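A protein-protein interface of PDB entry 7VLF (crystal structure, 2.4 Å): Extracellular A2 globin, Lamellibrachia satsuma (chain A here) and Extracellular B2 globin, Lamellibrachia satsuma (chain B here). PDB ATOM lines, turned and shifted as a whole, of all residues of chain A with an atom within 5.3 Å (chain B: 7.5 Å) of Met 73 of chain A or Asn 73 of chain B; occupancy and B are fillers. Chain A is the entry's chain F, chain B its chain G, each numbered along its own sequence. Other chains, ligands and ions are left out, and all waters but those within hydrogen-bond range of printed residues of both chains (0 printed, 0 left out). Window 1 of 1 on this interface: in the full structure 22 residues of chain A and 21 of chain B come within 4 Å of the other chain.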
ATOM      1  N   LEU A  68     -14.456  15.058 -31.702  1.00  0.00           N
ATOM      2  CA  LEU A  68     -14.767  16.249 -32.488  1.00  0.00           C
ATOM      3  C   LEU A  68     -14.547  17.515 -31.671  1.00  0.00           C
ATOM      4  O   LEU A  68     -13.898  18.462 -32.131  1.00  0.00           O
ATOM      5  CB  LEU A  68     -16.207  16.187 -33.000  1.00  0.00           C
ATOM      6  CG  LEU A  68     -16.503  15.292 -34.202  1.00  0.00           C
ATOM      7  CD1 LEU A  68     -17.808  15.723 -34.852  1.00  0.00           C
ATOM      8  CD2 LEU A  68     -15.360  15.331 -35.204  1.00  0.00           C
ATOM      9  N   GLY A  69     -15.087  17.550 -30.450  1.00  0.00           N
ATOM     10  CA  GLY A  69     -14.861  18.677 -29.564  1.00  0.00           C
ATOM     11  C   GLY A  69     -13.406  18.891 -29.211  1.00  0.00           C
ATOM     12  O   GLY A  69     -13.012  20.018 -28.894  1.00  0.00           O
ATOM     13  N   GLY A  70     -12.597  17.835 -29.258  1.00  0.00           N
ATOM     14  CA  GLY A  70     -11.170  17.969 -29.047  1.00  0.00           C
ATOM     15  C   GLY A  70     -10.463  18.541 -30.258  1.00  0.00           C
ATOM     16  O   GLY A  70      -9.605  19.418 -30.131  1.00  0.00           O
ATOM     17  N   LEU A  71     -10.817  18.045 -31.446  1.00  0.00           N
ATOM     18  CA  LEU A  71     -10.228  18.582 -32.667  1.00  0.00           C
ATOM     19  C   LEU A  71     -10.626  20.035 -32.880  1.00  0.00           C
ATOM     20  O   LEU A  71      -9.864  20.808 -33.470  1.00  0.00           O
ATOM     21  CB  LEU A  71     -10.639  17.729 -33.866  1.00  0.00           C
ATOM     22  CG  LEU A  71     -10.049  18.125 -35.220  1.00  0.00           C
ATOM     23  CD1 LEU A  71      -8.534  18.192 -35.142  1.00  0.00           C
ATOM     24  CD2 LEU A  71     -10.489  17.146 -36.295  1.00  0.00           C
ATOM     25  N   ASP A  72     -11.814  20.419 -32.408  1.00  0.00           N
ATOM     26  CA  ASP A  72     -12.219  21.820 -32.436  1.00  0.00           C
ATOM     27  C   ASP A  72     -11.198  22.696 -31.722  1.00  0.00           C
ATOM     28  O   ASP A  72     -10.781  23.737 -32.243  1.00  0.00           O
ATOM     29  CB  ASP A  72     -13.601  21.966 -31.794  1.00  0.00           C
ATOM     30  CG  ASP A  72     -14.102  23.398 -31.787  1.00  0.00           C
ATOM     31  OD1 ASP A  72     -13.467  24.263 -32.424  1.00  0.00           O
ATOM     32  OD2 ASP A  72     -15.137  23.661 -31.140  1.00  0.00           O
ATOM     33  N   MET A  73     -10.781  22.283 -30.524  1.00  0.00           N
ATOM     34  CA  MET A  73      -9.831  23.078 -29.752  1.00  0.00           C
ATOM     35  C   MET A  73      -8.502  23.220 -30.481  1.00  0.00           C
ATOM     36  O   MET A  73      -7.895  24.296 -30.474  1.00  0.00           O
ATOM     37  CB  MET A  73      -9.620  22.449 -28.379  1.00  0.00           C
ATOM     38  CG  MET A  73     -10.875  22.380 -27.539  1.00  0.00           C
ATOM     39  SD  MET A  73     -10.460  21.946 -25.847  1.00  0.00           S
ATOM     40  CE  MET A  73      -9.074  23.047 -25.584  1.00  0.00           C
ATOM     41  N   CYS A  74      -8.032  22.141 -31.111  1.00  0.00           N
ATOM     42  CA  CYS A  74      -6.788  22.215 -31.869  1.00  0.00           C
ATOM     43  C   CYS A  74      -6.928  23.162 -33.051  1.00  0.00           C
ATOM     44  O   CYS A  74      -6.033  23.972 -33.322  1.00  0.00           O
ATOM     45  CB  CYS A  74      -6.376  20.824 -32.347  1.00  0.00           C
ATOM     46  SG  CYS A  74      -6.304  19.577 -31.045  1.00  0.00           S
ATOM     47  N   VAL A  75      -8.051  23.079 -33.764  1.00  0.00           N
ATOM     48  CA  VAL A  75      -8.277  23.964 -34.900  1.00  0.00           C
ATOM     49  C   VAL A  75      -8.475  25.399 -34.431  1.00  0.00           C
ATOM     50  O   VAL A  75      -7.973  26.345 -35.053  1.00  0.00           O
ATOM     51  CB  VAL A  75      -9.471  23.462 -35.731  1.00  0.00           C
ATOM     52  CG1 VAL A  75      -9.812  24.453 -36.830  1.00  0.00           C
ATOM     53  CG2 VAL A  75      -9.159  22.096 -36.323  1.00  0.00           C
ATOM     54  N   ALA A  76      -9.198  25.592 -33.325  1.00  0.00           N
ATOM     55  CA  ALA A  76      -9.439  26.941 -32.829  1.00  0.00           C
ATOM     56  C   ALA A  76      -8.171  27.605 -32.313  1.00  0.00           C
ATOM     57  O   ALA A  76      -8.127  28.835 -32.208  1.00  0.00           O
ATOM     58  CB  ALA A  76     -10.494  26.920 -31.725  1.00  0.00           C
ATOM     59  N   LEU A  77      -7.146  26.823 -31.987  1.00  0.00           N
ATOM     60  CA  LEU A  77      -5.898  27.348 -31.462  1.00  0.00           C
ATOM     61  C   LEU A  77      -4.767  27.312 -32.478  1.00  0.00           C
ATOM     62  O   LEU A  77      -3.613  27.547 -32.108  1.00  0.00           O
ATOM     63  CB  LEU A  77      -5.495  26.578 -30.204  1.00  0.00           C
ATOM     64  CG  LEU A  77      -6.357  26.864 -28.976  1.00  0.00           C
ATOM     65  CD1 LEU A  77      -5.891  26.032 -27.797  1.00  0.00           C
ATOM     66  CD2 LEU A  77      -6.317  28.348 -28.649  1.00  0.00           C
ATOM     67  N   LEU A  78      -5.068  27.028 -33.747  1.00  0.00           N
ATOM     68  CA  LEU A  78      -4.021  27.000 -34.763  1.00  0.00           C
ATOM     69  C   LEU A  78      -3.330  28.350 -34.896  1.00  0.00           C
ATOM     70  O   LEU A  78      -2.165  28.415 -35.301  1.00  0.00           O
ATOM     71  CB  LEU A  78      -4.600  26.574 -36.111  1.00  0.00           C
ATOM     72  CG  LEU A  78      -4.571  25.079 -36.437  1.00  0.00           C
ATOM     73  CD1 LEU A  78      -5.111  24.815 -37.837  1.00  0.00           C
ATOM     74  CD2 LEU A  78      -3.162  24.521 -36.292  1.00  0.00           C
ATOM     75  N   GLN A  87      -2.060  22.382 -25.612  1.00  0.00           N
ATOM     76  CA  GLN A  87      -3.198  21.483 -25.764  1.00  0.00           C
ATOM     77  C   GLN A  87      -2.803  20.203 -26.491  1.00  0.00           C
ATOM     78  O   GLN A  87      -3.294  19.120 -26.156  1.00  0.00           O
ATOM     79  CB  GLN A  87      -4.333  22.191 -26.501  1.00  0.00           C
ATOM     80  CG  GLN A  87      -5.609  21.374 -26.597  1.00  0.00           C
ATOM     81  CD  GLN A  87      -6.175  21.012 -25.236  1.00  0.00           C
ATOM     82  OE1 GLN A  87      -6.005  21.747 -24.263  1.00  0.00           O
ATOM     83  NE2 GLN A  87      -6.850  19.870 -25.161  1.00  0.00           N
ATOM     84  N   TRP B  17     -25.980  30.812 -27.146  1.00  0.00           N
ATOM     85  CA  TRP B  17     -24.608  30.342 -27.001  1.00  0.00           C
ATOM     86  C   TRP B  17     -23.923  30.174 -28.349  1.00  0.00           C
ATOM     87  O   TRP B  17     -22.704  30.357 -28.446  1.00  0.00           O
ATOM     88  CB  TRP B  17     -24.595  29.025 -26.231  1.00  0.00           C
ATOM     89  CG  TRP B  17     -23.248  28.387 -26.123  1.00  0.00           C
ATOM     90  CD1 TRP B  17     -22.715  27.449 -26.958  1.00  0.00           C
ATOM     91  CD2 TRP B  17     -22.265  28.630 -25.112  1.00  0.00           C
ATOM     92  NE1 TRP B  17     -21.458  27.095 -26.532  1.00  0.00           N
ATOM     93  CE2 TRP B  17     -21.158  27.807 -25.400  1.00  0.00           C
ATOM     94  CE3 TRP B  17     -22.211  29.465 -23.992  1.00  0.00           C
ATOM     95  CZ2 TRP B  17     -20.013  27.795 -24.610  1.00  0.00           C
ATOM     96  CZ3 TRP B  17     -21.075  29.451 -23.211  1.00  0.00           C
ATOM     97  CH2 TRP B  17     -19.991  28.623 -23.522  1.00  0.00           C
ATOM     98  N   TRP B  21     -20.131  31.737 -28.708  1.00  0.00           N
ATOM     99  CA  TRP B  21     -19.050  30.761 -28.753  1.00  0.00           C
ATOM    100  C   TRP B  21     -18.983  30.178 -30.154  1.00  0.00           C
ATOM    101  O   TRP B  21     -20.018  29.832 -30.733  1.00  0.00           O
ATOM    102  CB  TRP B  21     -19.259  29.654 -27.721  1.00  0.00           C
ATOM    103  CG  TRP B  21     -18.298  28.512 -27.840  1.00  0.00           C
ATOM    104  CD1 TRP B  21     -18.354  27.477 -28.728  1.00  0.00           C
ATOM    105  CD2 TRP B  21     -17.148  28.272 -27.022  1.00  0.00           C
ATOM    106  NE1 TRP B  21     -17.307  26.615 -28.522  1.00  0.00           N
ATOM    107  CE2 TRP B  21     -16.552  27.080 -27.479  1.00  0.00           C
ATOM    108  CE3 TRP B  21     -16.560  28.952 -25.949  1.00  0.00           C
ATOM    109  CZ2 TRP B  21     -15.400  26.553 -26.901  1.00  0.00           C
ATOM    110  CZ3 TRP B  21     -15.417  28.427 -25.381  1.00  0.00           C
ATOM    111  CH2 TRP B  21     -14.849  27.240 -25.855  1.00  0.00           C
ATOM    112  N   ALA B  23     -15.986  28.088 -33.122  1.00  0.00           N
ATOM    113  CA  ALA B  23     -14.650  27.597 -33.437  1.00  0.00           C
ATOM    114  C   ALA B  23     -13.822  28.660 -34.141  1.00  0.00           C
ATOM    115  O   ALA B  23     -12.637  28.835 -33.837  1.00  0.00           O
ATOM    116  CB  ALA B  23     -14.744  26.343 -34.299  1.00  0.00           C
ATOM    117  N   ARG B  29     -13.524  33.026 -27.231  1.00  0.00           N
ATOM    118  CA  ARG B  29     -13.602  31.889 -26.321  1.00  0.00           C
ATOM    119  C   ARG B  29     -12.808  32.147 -25.048  1.00  0.00           C
ATOM    120  O   ARG B  29     -13.291  31.897 -23.938  1.00  0.00           O
ATOM    121  CB  ARG B  29     -13.089  30.629 -27.015  1.00  0.00           C
ATOM    122  CG  ARG B  29     -13.747  30.301 -28.340  1.00  0.00           C
ATOM    123  CD  ARG B  29     -13.052  29.105 -28.958  1.00  0.00           C
ATOM    124  NE  ARG B  29     -13.984  28.165 -29.567  1.00  0.00           N
ATOM    125  CZ  ARG B  29     -13.739  26.866 -29.706  1.00  0.00           C
ATOM    126  NH1 ARG B  29     -12.599  26.355 -29.261  1.00  0.00           N
ATOM    127  NH2 ARG B  29     -14.639  26.076 -30.272  1.00  0.00           N
ATOM    128  N   ALA B  33     -13.813  32.381 -21.025  1.00  0.00           N
ATOM    129  CA  ALA B  33     -13.240  31.329 -20.193  1.00  0.00           C
ATOM    130  C   ALA B  33     -12.484  31.913 -19.004  1.00  0.00           C
ATOM    131  O   ALA B  33     -12.636  31.445 -17.869  1.00  0.00           O
ATOM    132  CB  ALA B  33     -12.321  30.445 -21.035  1.00  0.00           C
ATOM    133  N   LYS B  65      -4.630  28.737 -19.799  1.00  0.00           N
ATOM    134  CA  LYS B  65      -5.370  29.044 -21.018  1.00  0.00           C
ATOM    135  C   LYS B  65      -5.928  27.770 -21.641  1.00  0.00           C
ATOM    136  O   LYS B  65      -7.118  27.693 -21.965  1.00  0.00           O
ATOM    137  CB  LYS B  65      -4.469  29.771 -22.017  1.00  0.00           C
ATOM    138  CG  LYS B  65      -3.680  30.935 -21.449  1.00  0.00           C
ATOM    139  CD  LYS B  65      -4.410  32.253 -21.608  1.00  0.00           C
ATOM    140  CE  LYS B  65      -3.446  33.419 -21.442  1.00  0.00           C
ATOM    141  NZ  LYS B  65      -4.099  34.744 -21.623  1.00  0.00           N
ATOM    142  N   ALA B  66      -5.074  26.756 -21.808  1.00  0.00           N
ATOM    143  CA  ALA B  66      -5.522  25.490 -22.377  1.00  0.00           C
ATOM    144  C   ALA B  66      -6.607  24.854 -21.517  1.00  0.00           C
ATOM    145  O   ALA B  66      -7.583  24.307 -22.039  1.00  0.00           O
ATOM    146  CB  ALA B  66      -4.337  24.539 -22.537  1.00  0.00           C
ATOM    147  N   HIS B  67      -6.451  24.918 -20.193  1.00  0.00           N
ATOM    148  CA  HIS B  67      -7.490  24.414 -19.302  1.00  0.00           C
ATOM    149  C   HIS B  67      -8.783  25.194 -19.482  1.00  0.00           C
ATOM    150  O   HIS B  67      -9.870  24.610 -19.551  1.00  0.00           O
ATOM    151  CB  HIS B  67      -7.019  24.486 -17.850  1.00  0.00           C
ATOM    152  CG  HIS B  67      -8.104  24.213 -16.853  1.00  0.00           C
ATOM    153  ND1 HIS B  67      -8.460  22.938 -16.471  1.00  0.00           N
ATOM    154  CD2 HIS B  67      -8.913  25.053 -16.163  1.00  0.00           C
ATOM    155  CE1 HIS B  67      -9.438  23.005 -15.585  1.00  0.00           C
ATOM    156  NE2 HIS B  67      -9.732  24.276 -15.382  1.00  0.00           N
ATOM    157  N   CYS B  68      -8.682  26.525 -19.556  1.00  0.00           N
ATOM    158  CA  CYS B  68      -9.867  27.355 -19.746  1.00  0.00           C
ATOM    159  C   CYS B  68     -10.597  26.995 -21.034  1.00  0.00           C
ATOM    160  O   CYS B  68     -11.828  26.886 -21.050  1.00  0.00           O
ATOM    161  CB  CYS B  68      -9.471  28.830 -19.747  1.00  0.00           C
ATOM    162  SG  CYS B  68      -9.151  29.502 -18.108  1.00  0.00           S
ATOM    163  N   ILE B  69      -9.854  26.802 -22.123  1.00  0.00           N
ATOM    164  CA  ILE B  69     -10.495  26.446 -23.381  1.00  0.00           C
ATOM    165  C   ILE B  69     -11.022  25.018 -23.331  1.00  0.00           C
ATOM    166  O   ILE B  69     -12.002  24.688 -24.008  1.00  0.00           O
ATOM    167  CB  ILE B  69      -9.515  26.655 -24.546  1.00  0.00           C
ATOM    168  CG1 ILE B  69      -8.925  28.061 -24.472  1.00  0.00           C
ATOM    169  CG2 ILE B  69     -10.218  26.465 -25.881  1.00  0.00           C
ATOM    170  CD1 ILE B  69      -7.746  28.270 -25.376  1.00  0.00           C
ATOM    171  N   ARG B  70     -10.396  24.152 -22.529  1.00  0.00           N
ATOM    172  CA  ARG B  70     -10.894  22.788 -22.383  1.00  0.00           C
ATOM    173  C   ARG B  70     -12.225  22.757 -21.647  1.00  0.00           C
ATOM    174  O   ARG B  70     -13.148  22.039 -22.048  1.00  0.00           O
ATOM    175  CB  ARG B  70      -9.869  21.925 -21.647  1.00  0.00           C
ATOM    176  CG  ARG B  70      -8.760  21.372 -22.520  1.00  0.00           C
ATOM    177  CD  ARG B  70      -7.912  20.357 -21.769  1.00  0.00           C
ATOM    178  NE  ARG B  70      -7.164  20.955 -20.664  1.00  0.00           N
ATOM    179  CZ  ARG B  70      -5.900  21.361 -20.749  1.00  0.00           C
ATOM    180  NH1 ARG B  70      -5.236  21.237 -21.889  1.00  0.00           N
ATOM    181  NH2 ARG B  70      -5.299  21.891 -19.692  1.00  0.00           N
ATOM    182  N   VAL B  71     -12.341  23.528 -20.566  1.00  0.00           N
ATOM    183  CA  VAL B  71     -13.525  23.449 -19.719  1.00  0.00           C
ATOM    184  C   VAL B  71     -14.750  23.970 -20.457  1.00  0.00           C
ATOM    185  O   VAL B  71     -15.807  23.329 -20.469  1.00  0.00           O
ATOM    186  CB  VAL B  71     -13.289  24.213 -18.404  1.00  0.00           C
ATOM    187  CG1 VAL B  71     -14.558  24.240 -17.571  1.00  0.00           C
ATOM    188  CG2 VAL B  71     -12.157  23.571 -17.629  1.00  0.00           C
ATOM    189  N   VAL B  72     -14.628  25.139 -21.089  1.00  0.00           N
ATOM    190  CA  VAL B  72     -15.788  25.729 -21.745  1.00  0.00           C
ATOM    191  C   VAL B  72     -16.132  24.973 -23.020  1.00  0.00           C
ATOM    192  O   VAL B  72     -17.291  24.966 -23.453  1.00  0.00           O
ATOM    193  CB  VAL B  72     -15.543  27.224 -22.010  1.00  0.00           C
ATOM    194  CG1 VAL B  72     -16.857  27.929 -22.270  1.00  0.00           C
ATOM    195  CG2 VAL B  72     -14.837  27.852 -20.823  1.00  0.00           C
ATOM    196  N   ASN B  73     -15.147  24.319 -23.640  1.00  0.00           N
ATOM    197  CA  ASN B  73     -15.456  23.429 -24.753  1.00  0.00           C
ATOM    198  C   ASN B  73     -16.281  22.237 -24.288  1.00  0.00           C
ATOM    199  O   ASN B  73     -17.096  21.710 -25.054  1.00  0.00           O
ATOM    200  CB  ASN B  73     -14.171  22.953 -25.426  1.00  0.00           C
ATOM    201  CG  ASN B  73     -14.436  22.141 -26.674  1.00  0.00           C
ATOM    202  OD1 ASN B  73     -14.520  22.685 -27.775  1.00  0.00           O
ATOM    203  ND2 ASN B  73     -14.572  20.830 -26.510  1.00  0.00           N
ATOM    204  N   GLY B  74     -16.078  21.797 -23.045  1.00  0.00           N
ATOM    205  CA  GLY B  74     -16.949  20.781 -22.481  1.00  0.00           C
ATOM    206  C   GLY B  74     -18.381  21.263 -22.351  1.00  0.00           C
ATOM    207  O   GLY B  74     -19.325  20.514 -22.611  1.00  0.00           O
ATOM    208  N   LEU B  75     -18.562  22.522 -21.947  1.00  0.00           N
ATOM    209  CA  LEU B  75     -19.903  23.099 -21.921  1.00  0.00           C
ATOM    210  C   LEU B  75     -20.449  23.273 -23.332  1.00  0.00           C
ATOM    211  O   LEU B  75     -21.651  23.092 -23.564  1.00  0.00           O
ATOM    212  CB  LEU B  75     -19.885  24.435 -21.180  1.00  0.00           C
ATOM    213  CG  LEU B  75     -21.232  25.147 -21.051  1.00  0.00           C
ATOM    214  CD1 LEU B  75     -22.223  24.280 -20.288  1.00  0.00           C
ATOM    215  CD2 LEU B  75     -21.059  26.493 -20.373  1.00  0.00           C
ATOM    216  N   ASP B  76     -19.582  23.626 -24.284  1.00  0.00           N
ATOM    217  CA  ASP B  76     -19.996  23.698 -25.683  1.00  0.00           C
ATOM    218  C   ASP B  76     -20.573  22.368 -26.145  1.00  0.00           C
ATOM    219  O   ASP B  76     -21.662  22.316 -26.730  1.00  0.00           O
ATOM    220  CB  ASP B  76     -18.810  24.103 -26.559  1.00  0.00           C
ATOM    221  CG  ASP B  76     -19.081  23.889 -28.037  1.00  0.00           C
ATOM    222  OD1 ASP B  76     -19.703  24.771 -28.660  1.00  0.00           O
ATOM    223  OD2 ASP B  76     -18.682  22.833 -28.573  1.00  0.00           O
ATOM    224  N   SER B  77     -19.849  21.277 -25.891  1.00  0.00           N
ATOM    225  CA  SER B  77     -20.379  19.955 -26.197  1.00  0.00           C
ATOM    226  C   SER B  77     -21.609  19.650 -25.355  1.00  0.00           C
ATOM    227  O   SER B  77     -22.556  19.016 -25.832  1.00  0.00           O
ATOM    228  CB  SER B  77     -19.299  18.897 -25.978  1.00  0.00           C
ATOM    229  OG  SER B  77     -18.230  19.070 -26.891  1.00  0.00           O
ATOM    230  N   ALA B  78     -21.619  20.107 -24.101  1.00  0.00           N
ATOM    231  CA  ALA B  78     -22.767  19.865 -23.232  1.00  0.00           C
ATOM    232  C   ALA B  78     -24.006  20.587 -23.745  1.00  0.00           C
ATOM    233  O   ALA B  78     -25.086  19.995 -23.852  1.00  0.00           O
ATOM    234  CB  ALA B  78     -22.443  20.299 -21.803  1.00  0.00           C
ATOM    235  N   ILE B  79     -23.869  21.875 -24.068  1.00  0.00           N
ATOM    236  CA  ILE B  79     -25.003  22.631 -24.593  1.00  0.00           C
ATOM    237  C   ILE B  79     -25.434  22.074 -25.942  1.00  0.00           C
ATOM    238  O   ILE B  79     -26.630  21.990 -26.245  1.00  0.00           O
ATOM    239  CB  ILE B  79     -24.652  24.126 -24.682  1.00  0.00           C
ATOM    240  CG1 ILE B  79     -24.372  24.688 -23.290  1.00  0.00           C
ATOM    241  CG2 ILE B  79     -25.776  24.902 -25.350  1.00  0.00           C
ATOM    242  CD1 ILE B  79     -24.032  26.157 -23.290  1.00  0.00           C
ATOM    243  N   GLN B  91     -22.347  11.525 -22.060  1.00  0.00           N
ATOM    244  CA  GLN B  91     -21.287  12.520 -21.939  1.00  0.00           C
ATOM    245  C   GLN B  91     -21.170  13.026 -20.507  1.00  0.00           C
ATOM    246  O   GLN B  91     -20.058  13.179 -19.988  1.00  0.00           O
ATOM    247  CB  GLN B  91     -21.542  13.679 -22.905  1.00  0.00           C
ATOM    248  CG  GLN B  91     -20.585  14.854 -22.764  1.00  0.00           C
ATOM    249  CD  GLN B  91     -19.241  14.611 -23.422  1.00  0.00           C
ATOM    250  OE1 GLN B  91     -18.840  13.472 -23.662  1.00  0.00           O
ATOM    251  NE2 GLN B  91     -18.533  15.693 -23.717  1.00  0.00           N
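SD of Met 73 of chain A lies close to O of Ile 69 of chain B, 3.6 Å away. The side-chain amide oxygen of Gln 87 of chain A is in hydrogen-bond range of the guanidinium group of Arg 70 of chain B. The side-chain carboxylate of Asp 72 of chain A is in salt-bridge range of the guanidinium group of Arg 29 of chain B (2.6 Å). ND2 of Asn 73 of chain B is in hydrogen-bond range of O of Gly 69 of chain A (3.0 Å).
O of Asn 73 of chain B is in hydrogen-bond range of OG of Ser 77 of chain B, at 3.4 Å.
Ala 23 of chain B touches Asp 72 of chain A. OD2 of Asp 72 of chain A touches OD1 of Asn 73 of chain B (3.6 Å). Arg 70 of chain B touches Met 73 of chain A. Met 73 of chain A touches Asn 73 of chain B (CG to OD1, 3.7 Å). Ala 76 of chain A touches Ala 23 of chain B (CB to O, 3.6 Å). Ala 76 of chain A touches Arg 29 of chain B. Leu 77 of chain A touches Ile 69 of chain B. Ala 66 of chain B touches Gln 87 of chain A.
Printed residues of chain B within 4 Å of Gly 69 of chain A: Asn 73 (3.0 Å). Met 73 of chain A touches three residues of chain B. Of the printed residues of chain B, Leu 77 of chain A touches Ile 69. Printed residues of chain B within 4 Å of Gln 87 of chain A: Ala 66 and Arg 70. Of the printed residues of chain A, Ala 66 of chain B touches Gln 87 (3.7 Å). Of the printed residues of chain A, Arg 70 of chain B touches Met 73 and Gln 87. Asn 73 of chain B touches just these residues of chain A: Gly 69 (3.0 Å), Asp 72 (3.6 Å) and Met 73 (3.7 Å). The nearest residue of chain B that does not touch Met 73 of chain A is Ala 66 of chain B (4.05 Å). The nearest residue of chain A that does not touch Asn 73 of chain B is Gly 70 of chain A (4.5 Å).
Hydrophobic or aromatic side chains of chain A that line the printed part of chain B: Met 73, Ala 76 and Leu 77. Of the 21 printed residues of chain B, 6 touch a printed residue of chain A. Printed residues of chain B that touch a printed residue of chain A: Ala 23, Arg 29, Ala 66, Ile 69, Arg 70 and Asn 73. Hydrophobic or aromatic side chains of chain B that line the printed part of chain A: Ala 23, Ala 66 and Ile 69. Along chain B the printed residues that touch a printed residue of chain A span positions 23 to 73. Among the printed residues, Asp or Glu carboxylates within 4 Å of a Lys or Arg side-chain nitrogen of the other chain: Asp 72 of chain A with Arg 29 of chain B.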
